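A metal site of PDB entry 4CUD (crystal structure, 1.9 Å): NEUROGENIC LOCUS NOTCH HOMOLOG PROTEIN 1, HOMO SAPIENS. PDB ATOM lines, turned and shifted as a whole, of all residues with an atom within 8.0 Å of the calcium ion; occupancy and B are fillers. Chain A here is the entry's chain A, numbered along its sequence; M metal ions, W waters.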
ATOM      1  N   GLN A  34      25.566 -26.514   8.723  1.00  0.00           N
ATOM      2  CA  GLN A  34      24.790 -25.825   9.749  1.00  0.00           C
ATOM      3  C   GLN A  34      25.021 -26.449  11.122  1.00  0.00           C
ATOM      4  O   GLN A  34      24.989 -27.671  11.255  1.00  0.00           O
ATOM      5  CB  GLN A  34      23.303 -25.859   9.396  1.00  0.00           C
ATOM      6  CG  GLN A  34      22.424 -25.126  10.391  1.00  0.00           C
ATOM      7  CD  GLN A  34      21.236 -24.449   9.730  1.00  0.00           C
ATOM      8  OE1 GLN A  34      20.878 -24.779   8.594  1.00  0.00           O
ATOM      9  NE2 GLN A  34      20.633 -23.491  10.424  1.00  0.00           N
ATOM     10  N   GLY A  35      25.297 -25.617  12.117  1.00  0.00           N
ATOM     11  CA  GLY A  35      25.526 -26.091  13.480  1.00  0.00           C
ATOM     12  C   GLY A  35      26.985 -26.283  13.849  1.00  0.00           C
ATOM     13  O   GLY A  35      27.306 -26.669  14.962  1.00  0.00           O
ATOM     14  N   TYR A  36      27.870 -25.990  12.903  1.00  0.00           N
ATOM     15  CA  TYR A  36      29.305 -26.036  13.153  1.00  0.00           C
ATOM     16  C   TYR A  36      29.985 -24.675  12.993  1.00  0.00           C
ATOM     17  O   TYR A  36      29.690 -23.941  12.062  1.00  0.00           O
ATOM     18  CB  TYR A  36      29.945 -27.103  12.257  1.00  0.00           C
ATOM     19  CG  TYR A  36      29.452 -28.484  12.589  1.00  0.00           C
ATOM     20  CD1 TYR A  36      29.880 -29.137  13.742  1.00  0.00           C
ATOM     21  CD2 TYR A  36      28.515 -29.134  11.767  1.00  0.00           C
ATOM     22  CE1 TYR A  36      29.411 -30.400  14.061  1.00  0.00           C
ATOM     23  CE2 TYR A  36      28.055 -30.410  12.082  1.00  0.00           C
ATOM     24  CZ  TYR A  36      28.511 -31.032  13.225  1.00  0.00           C
ATOM     25  OH  TYR A  36      28.058 -32.289  13.566  1.00  0.00           O
ATOM     26  N   ILE A  43      33.971 -26.644  16.031  1.00  0.00           N
ATOM     27  CA  ILE A  43      33.055 -26.542  17.155  1.00  0.00           C
ATOM     28  C   ILE A  43      31.626 -26.873  16.778  1.00  0.00           C
ATOM     29  O   ILE A  43      31.054 -26.306  15.841  1.00  0.00           O
ATOM     30  CB  ILE A  43      33.104 -25.142  17.812  1.00  0.00           C
ATOM     31  CG1 ILE A  43      34.550 -24.768  18.164  1.00  0.00           C
ATOM     32  CG2 ILE A  43      32.234 -25.129  19.070  1.00  0.00           C
ATOM     33  CD1 ILE A  43      34.714 -23.320  18.518  1.00  0.00           C
ATOM     34  N   ASP A  44      31.073 -27.824  17.511  1.00  0.00           N
ATOM     35  CA  ASP A  44      29.659 -28.122  17.462  1.00  0.00           C
ATOM     36  C   ASP A  44      29.016 -27.063  18.353  1.00  0.00           C
ATOM     37  O   ASP A  44      29.135 -27.125  19.584  1.00  0.00           O
ATOM     38  CB  ASP A  44      29.430 -29.515  18.030  1.00  0.00           C
ATOM     39  CG  ASP A  44      27.953 -29.865  18.190  1.00  0.00           C
ATOM     40  OD1 ASP A  44      27.076 -29.013  17.918  1.00  0.00           O
ATOM     41  OD2 ASP A  44      27.691 -31.018  18.602  1.00  0.00           O
ATOM     42  N   VAL A  45      28.349 -26.099  17.724  1.00  0.00           N
ATOM     43  CA  VAL A  45      27.634 -25.040  18.443  1.00  0.00           C
ATOM     44  C   VAL A  45      26.702 -25.641  19.506  1.00  0.00           C
ATOM     45  O   VAL A  45      26.030 -26.634  19.245  1.00  0.00           O
ATOM     46  CB  VAL A  45      26.800 -24.169  17.483  1.00  0.00           C
ATOM     47  CG1 VAL A  45      25.872 -23.225  18.233  1.00  0.00           C
ATOM     48  CG2 VAL A  45      27.704 -23.382  16.539  1.00  0.00           C
ATOM     49  N   ASN A  46      26.700 -25.062  20.700  1.00  0.00           N
ATOM     50  CA  ASN A  46      25.712 -25.443  21.704  1.00  0.00           C
ATOM     51  C   ASN A  46      24.457 -24.599  21.582  1.00  0.00           C
ATOM     52  O   ASN A  46      24.396 -23.469  22.085  1.00  0.00           O
ATOM     53  CB  ASN A  46      26.297 -25.335  23.114  1.00  0.00           C
ATOM     54  CG  ASN A  46      25.339 -25.846  24.183  1.00  0.00           C
ATOM     55  OD1 ASN A  46      24.233 -26.283  23.886  1.00  0.00           O
ATOM     56  ND2 ASN A  46      25.752 -25.758  25.439  1.00  0.00           N
ATOM     57  N   GLU A  47      23.423 -25.139  20.935  1.00  0.00           N
ATOM     58  CA  GLU A  47      22.171 -24.389  20.762  1.00  0.00           C
ATOM     59  C   GLU A  47      21.406 -24.163  22.083  1.00  0.00           C
ATOM     60  O   GLU A  47      20.444 -23.396  22.119  1.00  0.00           O
ATOM     61  CB  GLU A  47      21.269 -25.037  19.711  1.00  0.00           C
ATOM     62  CG  GLU A  47      21.736 -24.826  18.279  1.00  0.00           C
ATOM     63  CD  GLU A  47      22.891 -25.738  17.866  1.00  0.00           C
ATOM     64  OE1 GLU A  47      23.181 -26.727  18.584  1.00  0.00           O
ATOM     65  OE2 GLU A  47      23.512 -25.463  16.827  1.00  0.00           O
ATOM     66  N   CYS A  48      21.846 -24.850  23.136  1.00  0.00           N
ATOM     67  CA  CYS A  48      21.239 -24.764  24.472  1.00  0.00           C
ATOM     68  C   CYS A  48      21.914 -23.749  25.402  1.00  0.00           C
ATOM     69  O   CYS A  48      21.442 -23.521  26.513  1.00  0.00           O
ATOM     70  CB  CYS A  48      21.257 -26.140  25.146  1.00  0.00           C
ATOM     71  SG  CYS A  48      20.209 -27.365  24.313  1.00  0.00           S
ATOM     72  N   LEU A  60      17.860 -30.352  24.512  1.00  0.00           N
ATOM     73  CA  LEU A  60      18.726 -31.262  23.766  1.00  0.00           C
ATOM     74  C   LEU A  60      19.563 -30.470  22.771  1.00  0.00           C
ATOM     75  O   LEU A  60      19.021 -29.764  21.912  1.00  0.00           O
ATOM     76  CB  LEU A  60      17.897 -32.329  23.042  1.00  0.00           C
ATOM     77  CG  LEU A  60      16.915 -33.146  23.917  1.00  0.00           C
ATOM     78  CD1 LEU A  60      15.946 -33.938  23.048  1.00  0.00           C
ATOM     79  CD2 LEU A  60      17.644 -34.067  24.888  1.00  0.00           C
ATOM     80  N   ASP A  61      20.884 -30.562  22.922  1.00  0.00           N
ATOM     81  CA  ASP A  61      21.813 -29.859  22.071  1.00  0.00           C
ATOM     82  C   ASP A  61      22.138 -30.738  20.850  1.00  0.00           C
ATOM     83  O   ASP A  61      22.886 -31.713  20.953  1.00  0.00           O
ATOM     84  CB  ASP A  61      23.072 -29.475  22.849  1.00  0.00           C
ATOM     85  CG  ASP A  61      24.189 -28.935  21.969  1.00  0.00           C
ATOM     86  OD1 ASP A  61      23.913 -28.472  20.837  1.00  0.00           O
ATOM     87  OD2 ASP A  61      25.360 -28.987  22.417  1.00  0.00           O
ATOM     88  N   GLN A  62      21.574 -30.372  19.703  1.00  0.00           N
ATOM     89  CA  GLN A  62      21.613 -31.206  18.510  1.00  0.00           C
ATOM     90  C   GLN A  62      22.404 -30.538  17.401  1.00  0.00           C
ATOM     91  O   GLN A  62      22.876 -29.402  17.562  1.00  0.00           O
ATOM     92  CB  GLN A  62      20.180 -31.533  18.063  1.00  0.00           C
ATOM     93  CG  GLN A  62      19.361 -32.254  19.134  1.00  0.00           C
ATOM     94  CD  GLN A  62      17.874 -32.264  18.847  1.00  0.00           C
ATOM     95  OE1 GLN A  62      17.395 -31.551  17.973  1.00  0.00           O
ATOM     96  NE2 GLN A  62      17.132 -33.076  19.589  1.00  0.00           N
ATOM     97  N   ILE A  63      22.572 -31.233  16.282  1.00  0.00           N
ATOM     98  CA  ILE A  63      23.304 -30.680  15.140  1.00  0.00           C
ATOM     99  C   ILE A  63      22.469 -29.604  14.465  1.00  0.00           C
ATOM    100  O   ILE A  63      21.469 -29.903  13.794  1.00  0.00           O
ATOM    101  CB  ILE A  63      23.720 -31.763  14.120  1.00  0.00           C
ATOM    102  CG1 ILE A  63      24.527 -32.869  14.824  1.00  0.00           C
ATOM    103  CG2 ILE A  63      24.559 -31.147  13.006  1.00  0.00           C
ATOM    104  CD1 ILE A  63      24.708 -34.134  13.997  1.00  0.00           C
ATOM    105  N   GLY A  64      22.879 -28.353  14.635  1.00  0.00           N
ATOM    106  CA  GLY A  64      22.211 -27.242  13.978  1.00  0.00           C
ATOM    107  C   GLY A  64      20.900 -26.812  14.619  1.00  0.00           C
ATOM    108  O   GLY A  64      20.207 -25.934  14.079  1.00  0.00           O
ATOM    109  N   GLU A  65      20.552 -27.414  15.759  1.00  0.00           N
ATOM    110  CA  GLU A  65      19.276 -27.129  16.420  1.00  0.00           C
ATOM    111  C   GLU A  65      19.219 -27.552  17.891  1.00  0.00           C
ATOM    112  O   GLU A  65      20.086 -28.283  18.368  1.00  0.00           O
ATOM    113  CB  GLU A  65      18.101 -27.765  15.652  1.00  0.00           C
ATOM    114  CG  GLU A  65      18.179 -29.263  15.442  1.00  0.00           C
ATOM    115  CD  GLU A  65      17.107 -29.779  14.490  1.00  0.00           C
ATOM    116  OE1 GLU A  65      15.934 -29.393  14.624  1.00  0.00           O
ATOM    117  OE2 GLU A  65      17.438 -30.589  13.603  1.00  0.00           O
ATOM    118  N   PHE A  66      18.220 -27.043  18.608  1.00  0.00           N
ATOM    119  CA  PHE A  66      17.858 -27.573  19.914  1.00  0.00           C
ATOM    120  C   PHE A  66      16.436 -28.124  19.873  1.00  0.00           C
ATOM    121  O   PHE A  66      15.659 -27.747  18.989  1.00  0.00           O
ATOM    122  CB  PHE A  66      17.995 -26.508  21.020  1.00  0.00           C
ATOM    123  CG  PHE A  66      16.957 -25.401  20.944  1.00  0.00           C
ATOM    124  CD1 PHE A  66      15.719 -25.525  21.581  1.00  0.00           C
ATOM    125  CD2 PHE A  66      17.245 -24.231  20.260  1.00  0.00           C
ATOM    126  CE1 PHE A  66      14.781 -24.509  21.515  1.00  0.00           C
ATOM    127  CE2 PHE A  66      16.305 -23.202  20.192  1.00  0.00           C
ATOM    128  CZ  PHE A  66      15.074 -23.347  20.820  1.00  0.00           C
HETATM  129 CA    CA M   1      24.827 -28.478  18.602  1.00  0.00          CA
HETATM  130  O   HOH W   1      25.028 -27.629  16.351  1.00  0.00           O
HETATM  131  O   HOH W   2      25.060 -30.922  19.149  1.00  0.00           O
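Within 4 Å of the calcium ion: Asp 44, Val 45, Glu 47, Asp 61 and Gln 62.
Water W2 bridges OD2 of Asp 44 (2.7 Å) and O of Asp 61 (2.9 Å).
Water W1 lies within hydrogen-bond range of the side-chain carboxylate (OE2) of Glu 47, the backbone carbonyl oxygen (O) of Gly 35 and the backbone NH (N) of Gly 64.
O of Val 45 is bound to the calcium ion, at 2.3 Å.
The backbone carbonyl oxygen (O) of Gln 62 is bound to the calcium ion (2.4 Å).
The calcium ion is bound by the side-chain carboxylate (OE1) of Glu 47 (2.4 Å).
The side-chain carboxylate (OD1) of Asp 44 binds the calcium ion, at 2.4 Å.
Water W1 binds the calcium ion (2.4 Å).
The calcium ion is bound by OD1 of Asp 61 (2.4 Å).
Water W2 binds the calcium ion (2.5 Å).
The calcium ion has seven donor atoms within binding distance.
N of Val 45 sits at hydrogen-bond distance from O of Gly 35 (3.0 Å).
OD2 of Asp 61 sits close to OD1 of Asn 46 (3.3 Å).
The side-chain sulfur of Cys 48 sits at hydrogen-bond distance from the backbone NH of Asp 61.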
